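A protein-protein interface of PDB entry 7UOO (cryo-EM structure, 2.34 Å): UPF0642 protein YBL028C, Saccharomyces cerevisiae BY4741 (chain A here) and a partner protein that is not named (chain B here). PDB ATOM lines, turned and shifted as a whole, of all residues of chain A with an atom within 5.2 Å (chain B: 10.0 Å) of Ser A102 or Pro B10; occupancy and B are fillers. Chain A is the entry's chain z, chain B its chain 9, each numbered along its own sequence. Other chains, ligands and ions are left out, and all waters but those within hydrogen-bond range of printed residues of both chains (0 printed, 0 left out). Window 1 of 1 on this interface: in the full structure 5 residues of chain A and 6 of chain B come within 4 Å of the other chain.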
ATOM      1  N   GLN A  96     -32.624 -21.680 -18.247  1.00  0.00           N
ATOM      2  CA  GLN A  96     -32.141 -22.308 -19.473  1.00  0.00           C
ATOM      3  C   GLN A  96     -30.752 -21.804 -19.846  1.00  0.00           C
ATOM      4  O   GLN A  96     -29.890 -22.590 -20.252  1.00  0.00           O
ATOM      5  CB  GLN A  96     -33.122 -22.063 -20.617  1.00  0.00           C
ATOM      6  CG  GLN A  96     -34.340 -22.963 -20.589  1.00  0.00           C
ATOM      7  CD  GLN A  96     -35.229 -22.761 -21.793  1.00  0.00           C
ATOM      8  OE1 GLN A  96     -35.008 -21.855 -22.594  1.00  0.00           O
ATOM      9  NE2 GLN A  96     -36.239 -23.607 -21.931  1.00  0.00           N
ATOM     10  N   LYS A 100     -27.557 -24.231 -19.717  1.00  0.00           N
ATOM     11  CA  LYS A 100     -27.142 -24.468 -21.102  1.00  0.00           C
ATOM     12  C   LYS A 100     -28.023 -25.520 -21.775  1.00  0.00           C
ATOM     13  O   LYS A 100     -27.540 -26.447 -22.427  1.00  0.00           O
ATOM     14  CB  LYS A 100     -25.662 -24.855 -21.175  1.00  0.00           C
ATOM     15  CG  LYS A 100     -24.732 -23.818 -20.578  1.00  0.00           C
ATOM     16  CD  LYS A 100     -23.313 -24.342 -20.459  1.00  0.00           C
ATOM     17  CE  LYS A 100     -22.373 -23.246 -19.986  1.00  0.00           C
ATOM     18  NZ  LYS A 100     -22.877 -22.584 -18.752  1.00  0.00           N
ATOM     19  N   THR A 101     -29.335 -25.366 -21.612  1.00  0.00           N
ATOM     20  CA  THR A 101     -30.325 -26.278 -22.172  1.00  0.00           C
ATOM     21  C   THR A 101     -31.334 -25.522 -23.027  1.00  0.00           C
ATOM     22  O   THR A 101     -32.530 -25.823 -23.018  1.00  0.00           O
ATOM     23  CB  THR A 101     -31.043 -27.057 -21.071  1.00  0.00           C
ATOM     24  OG1 THR A 101     -31.605 -26.139 -20.124  1.00  0.00           O
ATOM     25  CG2 THR A 101     -30.080 -27.995 -20.356  1.00  0.00           C
ATOM     26  N   SER A 102     -30.869 -24.532 -23.781  1.00  0.00           N
ATOM     27  CA  SER A 102     -31.733 -23.724 -24.629  1.00  0.00           C
ATOM     28  C   SER A 102     -31.734 -24.259 -26.055  1.00  0.00           C
ATOM     29  O   SER A 102     -30.705 -24.716 -26.559  1.00  0.00           O
ATOM     30  CB  SER A 102     -31.287 -22.261 -24.623  1.00  0.00           C
ATOM     31  OG  SER A 102     -32.046 -21.496 -25.540  1.00  0.00           O
ATOM     32  N   PHE A 103     -32.902 -24.205 -26.699  1.00  0.00           N
ATOM     33  CA  PHE A 103     -33.030 -24.694 -28.068  1.00  0.00           C
ATOM     34  C   PHE A 103     -32.447 -23.732 -29.092  1.00  0.00           C
ATOM     35  O   PHE A 103     -31.906 -24.176 -30.110  1.00  0.00           O
ATOM     36  CB  PHE A 103     -34.499 -24.956 -28.405  1.00  0.00           C
ATOM     37  CG  PHE A 103     -34.997 -26.296 -27.956  1.00  0.00           C
ATOM     38  CD1 PHE A 103     -35.522 -26.466 -26.687  1.00  0.00           C
ATOM     39  CD2 PHE A 103     -34.946 -27.386 -28.806  1.00  0.00           C
ATOM     40  CE1 PHE A 103     -35.983 -27.700 -26.273  1.00  0.00           C
ATOM     41  CE2 PHE A 103     -35.407 -28.620 -28.397  1.00  0.00           C
ATOM     42  CZ  PHE A 103     -35.924 -28.779 -27.128  1.00  0.00           C
ATOM     43  N   THR A 104     -32.539 -22.427 -28.847  1.00  0.00           N
ATOM     44  CA  THR A 104     -32.223 -21.439 -29.865  1.00  0.00           C
ATOM     45  C   THR A 104     -31.077 -20.505 -29.510  1.00  0.00           C
ATOM     46  O   THR A 104     -30.620 -19.768 -30.389  1.00  0.00           O
ATOM     47  CB  THR A 104     -33.463 -20.587 -30.182  1.00  0.00           C
ATOM     48  OG1 THR A 104     -34.011 -20.065 -28.967  1.00  0.00           O
ATOM     49  CG2 THR A 104     -34.517 -21.420 -30.889  1.00  0.00           C
ATOM     50  N   ARG A 105     -30.601 -20.500 -28.271  1.00  0.00           N
ATOM     51  CA  ARG A 105     -29.606 -19.534 -27.827  1.00  0.00           C
ATOM     52  C   ARG A 105     -28.392 -20.253 -27.260  1.00  0.00           C
ATOM     53  O   ARG A 105     -28.528 -21.128 -26.398  1.00  0.00           O
ATOM     54  CB  ARG A 105     -30.200 -18.585 -26.783  1.00  0.00           C
ATOM     55  CG  ARG A 105     -31.322 -17.716 -27.321  1.00  0.00           C
ATOM     56  CD  ARG A 105     -31.993 -16.916 -26.222  1.00  0.00           C
ATOM     57  NE  ARG A 105     -32.969 -15.975 -26.762  1.00  0.00           N
ATOM     58  CZ  ARG A 105     -32.684 -14.735 -27.133  1.00  0.00           C
ATOM     59  NH1 ARG A 105     -31.459 -14.246 -27.027  1.00  0.00           N
ATOM     60  NH2 ARG A 105     -33.650 -13.966 -27.625  1.00  0.00           N
ATOM     61  N   PRO B   2     -26.062 -34.934 -28.996  1.00  0.00           N
ATOM     62  CA  PRO B   2     -27.443 -34.525 -28.721  1.00  0.00           C
ATOM     63  C   PRO B   2     -28.461 -35.605 -29.076  1.00  0.00           C
ATOM     64  O   PRO B   2     -28.159 -36.511 -29.848  1.00  0.00           O
ATOM     65  CB  PRO B   2     -27.623 -33.291 -29.609  1.00  0.00           C
ATOM     66  CG  PRO B   2     -26.663 -33.493 -30.724  1.00  0.00           C
ATOM     67  CD  PRO B   2     -25.474 -34.173 -30.111  1.00  0.00           C
ATOM     68  N   SER B   3     -29.658 -35.497 -28.509  1.00  0.00           N
ATOM     69  CA  SER B   3     -30.705 -36.474 -28.763  1.00  0.00           C
ATOM     70  C   SER B   3     -31.308 -36.284 -30.150  1.00  0.00           C
ATOM     71  O   SER B   3     -31.386 -35.171 -30.672  1.00  0.00           O
ATOM     72  CB  SER B   3     -31.799 -36.363 -27.704  1.00  0.00           C
ATOM     73  OG  SER B   3     -32.894 -37.204 -28.014  1.00  0.00           O
ATOM     74  N   SER B   6     -34.333 -33.930 -30.130  1.00  0.00           N
ATOM     75  CA  SER B   6     -34.091 -32.491 -29.987  1.00  0.00           C
ATOM     76  C   SER B   6     -32.601 -32.244 -30.230  1.00  0.00           C
ATOM     77  O   SER B   6     -31.792 -32.298 -29.302  1.00  0.00           O
ATOM     78  CB  SER B   6     -34.529 -31.996 -28.618  1.00  0.00           C
ATOM     79  OG  SER B   6     -33.890 -32.722 -27.584  1.00  0.00           O
ATOM     80  N   ILE B   7     -32.256 -31.939 -31.482  1.00  0.00           N
ATOM     81  CA  ILE B   7     -30.850 -31.789 -31.841  1.00  0.00           C
ATOM     82  C   ILE B   7     -30.315 -30.394 -31.548  1.00  0.00           C
ATOM     83  O   ILE B   7     -29.101 -30.230 -31.381  1.00  0.00           O
ATOM     84  CB  ILE B   7     -30.616 -32.127 -33.323  1.00  0.00           C
ATOM     85  CG1 ILE B   7     -31.551 -31.308 -34.212  1.00  0.00           C
ATOM     86  CG2 ILE B   7     -30.795 -33.618 -33.567  1.00  0.00           C
ATOM     87  CD1 ILE B   7     -31.128 -31.271 -35.654  1.00  0.00           C
ATOM     88  N   ASN B   8     -31.179 -29.384 -31.476  1.00  0.00           N
ATOM     89  CA  ASN B   8     -30.723 -28.028 -31.204  1.00  0.00           C
ATOM     90  C   ASN B   8     -30.438 -27.779 -29.727  1.00  0.00           C
ATOM     91  O   ASN B   8     -29.816 -26.763 -29.400  1.00  0.00           O
ATOM     92  CB  ASN B   8     -31.752 -27.016 -31.715  1.00  0.00           C
ATOM     93  CG  ASN B   8     -31.756 -26.900 -33.232  1.00  0.00           C
ATOM     94  OD1 ASN B   8     -30.740 -27.125 -33.884  1.00  0.00           O
ATOM     95  ND2 ASN B   8     -32.902 -26.548 -33.795  1.00  0.00           N
ATOM     96  N   ARG B   9     -30.865 -28.672 -28.833  1.00  0.00           N
ATOM     97  CA  ARG B   9     -30.637 -28.499 -27.406  1.00  0.00           C
ATOM     98  C   ARG B   9     -29.409 -29.283 -26.975  1.00  0.00           C
ATOM     99  O   ARG B   9     -29.343 -30.496 -27.225  1.00  0.00           O
ATOM    100  CB  ARG B   9     -31.854 -28.948 -26.606  1.00  0.00           C
ATOM    101  CG  ARG B   9     -31.661 -28.856 -25.099  1.00  0.00           C
ATOM    102  CD  ARG B   9     -32.964 -29.050 -24.346  1.00  0.00           C
ATOM    103  NE  ARG B   9     -33.517 -30.384 -24.532  1.00  0.00           N
ATOM    104  CZ  ARG B   9     -34.683 -30.784 -24.046  1.00  0.00           C
ATOM    105  NH1 ARG B   9     -35.453 -29.969 -23.345  1.00  0.00           N
ATOM    106  NH2 ARG B   9     -35.085 -32.031 -24.266  1.00  0.00           N
ATOM    107  N   PRO B  10     -28.420 -28.649 -26.346  1.00  0.00           N
ATOM    108  CA  PRO B  10     -27.247 -29.395 -25.875  1.00  0.00           C
ATOM    109  C   PRO B  10     -27.599 -30.318 -24.716  1.00  0.00           C
ATOM    110  O   PRO B  10     -28.301 -29.930 -23.779  1.00  0.00           O
ATOM    111  CB  PRO B  10     -26.273 -28.294 -25.435  1.00  0.00           C
ATOM    112  CG  PRO B  10     -26.802 -27.028 -26.033  1.00  0.00           C
ATOM    113  CD  PRO B  10     -28.282 -27.203 -26.115  1.00  0.00           C
ATOM    114  N   LYS B  11     -27.100 -31.550 -24.790  1.00  0.00           N
ATOM    115  CA  LYS B  11     -27.413 -32.580 -23.804  1.00  0.00           C
ATOM    116  C   LYS B  11     -26.181 -33.033 -23.030  1.00  0.00           C
ATOM    117  O   LYS B  11     -26.153 -32.925 -21.796  1.00  0.00           O
ATOM    118  CB  LYS B  11     -28.081 -33.758 -24.526  1.00  0.00           C
ATOM    119  CG  LYS B  11     -28.501 -34.929 -23.658  1.00  0.00           C
ATOM    120  CD  LYS B  11     -29.136 -36.004 -24.529  1.00  0.00           C
ATOM    121  CE  LYS B  11     -29.718 -37.143 -23.714  1.00  0.00           C
ATOM    122  NZ  LYS B  11     -30.780 -36.686 -22.779  1.00  0.00           N
ATOM    123  N   LEU B  12     -25.148 -33.517 -23.728  1.00  0.00           N
ATOM    124  CA  LEU B  12     -23.957 -34.032 -23.057  1.00  0.00           C
ATOM    125  C   LEU B  12     -23.212 -32.930 -22.315  1.00  0.00           C
ATOM    126  O   LEU B  12     -22.756 -33.138 -21.184  1.00  0.00           O
ATOM    127  CB  LEU B  12     -23.033 -34.708 -24.071  1.00  0.00           C
ATOM    128  CG  LEU B  12     -21.636 -35.075 -23.559  1.00  0.00           C
ATOM    129  CD1 LEU B  12     -21.700 -36.250 -22.603  1.00  0.00           C
ATOM    130  CD2 LEU B  12     -20.677 -35.356 -24.704  1.00  0.00           C
ATOM    131  N   THR B  13     -23.070 -31.755 -22.934  1.00  0.00           N
ATOM    132  CA  THR B  13     -22.344 -30.667 -22.287  1.00  0.00           C
ATOM    133  C   THR B  13     -23.072 -30.180 -21.041  1.00  0.00           C
ATOM    134  O   THR B  13     -22.436 -29.876 -20.026  1.00  0.00           O
ATOM    135  CB  THR B  13     -22.119 -29.516 -23.266  1.00  0.00           C
ATOM    136  OG1 THR B  13     -23.352 -29.175 -23.909  1.00  0.00           O
ATOM    137  CG2 THR B  13     -21.091 -29.903 -24.312  1.00  0.00           C
ATOM    138  N   SER B  14     -24.403 -30.103 -21.095  1.00  0.00           N
ATOM    139  CA  SER B  14     -25.168 -29.718 -19.913  1.00  0.00           C
ATOM    140  C   SER B  14     -25.026 -30.752 -18.802  1.00  0.00           C
ATOM    141  O   SER B  14     -24.867 -30.392 -17.627  1.00  0.00           O
ATOM    142  CB  SER B  14     -26.637 -29.515 -20.280  1.00  0.00           C
ATOM    143  OG  SER B  14     -27.184 -30.675 -20.873  1.00  0.00           O
ATOM    144  N   ASN B  15     -25.069 -32.043 -19.155  1.00  0.00           N
ATOM    145  CA  ASN B  15     -24.881 -33.087 -18.151  1.00  0.00           C
ATOM    146  C   ASN B  15     -23.503 -32.994 -17.503  1.00  0.00           C
ATOM    147  O   ASN B  15     -23.375 -33.105 -16.276  1.00  0.00           O
ATOM    148  CB  ASN B  15     -25.084 -34.468 -18.777  1.00  0.00           C
ATOM    149  CG  ASN B  15     -26.540 -34.770 -19.070  1.00  0.00           C
ATOM    150  OD1 ASN B  15     -27.436 -34.319 -18.361  1.00  0.00           O
ATOM    151  ND2 ASN B  15     -26.780 -35.546 -20.119  1.00  0.00           N
ATOM    152  N   LEU B  16     -22.462 -32.773 -18.312  1.00  0.00           N
ATOM    153  CA  LEU B  16     -21.107 -32.665 -17.775  1.00  0.00           C
ATOM    154  C   LEU B  16     -20.945 -31.426 -16.903  1.00  0.00           C
ATOM    155  O   LEU B  16     -20.267 -31.474 -15.870  1.00  0.00           O
ATOM    156  CB  LEU B  16     -20.087 -32.649 -18.912  1.00  0.00           C
ATOM    157  CG  LEU B  16     -19.958 -33.927 -19.741  1.00  0.00           C
ATOM    158  CD1 LEU B  16     -18.815 -33.803 -20.731  1.00  0.00           C
ATOM    159  CD2 LEU B  16     -19.777 -35.141 -18.841  1.00  0.00           C
ATOM    160  N   HIS B  17     -21.542 -30.304 -17.314  1.00  0.00           N
ATOM    161  CA  HIS B  17     -21.473 -29.085 -16.517  1.00  0.00           C
ATOM    162  C   HIS B  17     -22.141 -29.276 -15.160  1.00  0.00           C
ATOM    163  O   HIS B  17     -21.589 -28.879 -14.123  1.00  0.00           O
ATOM    164  CB  HIS B  17     -22.120 -27.935 -17.289  1.00  0.00           C
ATOM    165  CG  HIS B  17     -22.038 -26.612 -16.597  1.00  0.00           C
ATOM    166  ND1 HIS B  17     -20.872 -25.882 -16.523  1.00  0.00           N
ATOM    167  CD2 HIS B  17     -22.981 -25.881 -15.957  1.00  0.00           C
ATOM    168  CE1 HIS B  17     -21.098 -24.762 -15.862  1.00  0.00           C
ATOM    169  NE2 HIS B  17     -22.370 -24.737 -15.507  1.00  0.00           N
ATOM    170  N   HIS B  18     -23.319 -29.909 -15.150  1.00  0.00           N
ATOM    171  CA  HIS B  18     -24.001 -30.193 -13.891  1.00  0.00           C
ATOM    172  C   HIS B  18     -23.174 -31.123 -13.011  1.00  0.00           C
ATOM    173  O   HIS B  18     -23.090 -30.924 -11.793  1.00  0.00           O
ATOM    174  CB  HIS B  18     -25.377 -30.800 -14.167  1.00  0.00           C
ATOM    175  CG  HIS B  18     -26.129 -31.176 -12.930  1.00  0.00           C
ATOM    176  ND1 HIS B  18     -26.748 -30.246 -12.124  1.00  0.00           N
ATOM    177  CD2 HIS B  18     -26.355 -32.381 -12.356  1.00  0.00           C
ATOM    178  CE1 HIS B  18     -27.325 -30.862 -11.108  1.00  0.00           C
ATOM    179  NE2 HIS B  18     -27.103 -32.158 -11.226  1.00  0.00           N
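O of Asn B8 lies close to O of Phe A103 (3.4 Å).
The backbone carbonyl oxygen (O) of Gln A96 sits at hydrogen-bond distance from the backbone NH (N) of Thr A101 (3.1 Å). OG of Ser A102 sits close to N of Thr A104, at 3.5 Å. The side-chain hydroxyl of Ser A102 lies within hydrogen-bond range of the backbone NH of Arg A105, 3.2 Å away. The side-chain hydroxyl of Ser B14 sits at hydrogen-bond distance from the backbone carbonyl oxygen of Pro B10, 3.2 Å away. The backbone carbonyl oxygen (O) of Lys B11 sits at hydrogen-bond distance from the side-chain hydroxyl (OG) of Ser B14, at 2.6 Å.
Pro B10 touches just these residues of chain A: Lys A100 (3.7 Å) and Ser A102 (3.5 Å). Thr A101 touches just these residues of chain B: Arg B9 and Ser B14. Printed residues of chain B within 4 Å of Lys A100: Pro B10 (3.7 Å), Ser B14 (3.9 Å) and His B17 (3.9 Å). Of the printed residues of chain A, Ser B14 touches Lys A100 and Thr A101. Of the printed residues of chain A, His B17 touches Lys A100 (3.9 Å). Arg A105 touches none of the printed residues of chain B. The nearest printed residue of chain A that does not touch Arg B9 is Lys A100 (5.5 Å).
Lys A100 touches Pro B10. Ser B14 touches Lys A100 (CB to O, 3.9 Å). His B17 touches Lys A100 (NE2 to NZ, 3.9 Å). CD of Arg B9 touches O of Thr A101 (3.5 Å). CB of Ser B14 touches CG2 of Thr A101, at 3.8 Å. Asn B8 touches Ser A102 (O to O, 3.6 Å). CA of Arg B9 touches O of Ser A102, 3.9 Å away. Ser A102 touches Pro B10. Phe A103 touches Ser B6. Arg B9 touches Phe A103.
Printed residues of chain B that touch a printed residue of chain A: Ser B6, Asn B8, Arg B9, Pro B10, Ser B14 and His B17. Among the printed residues, 11 pairs touch across the chains.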
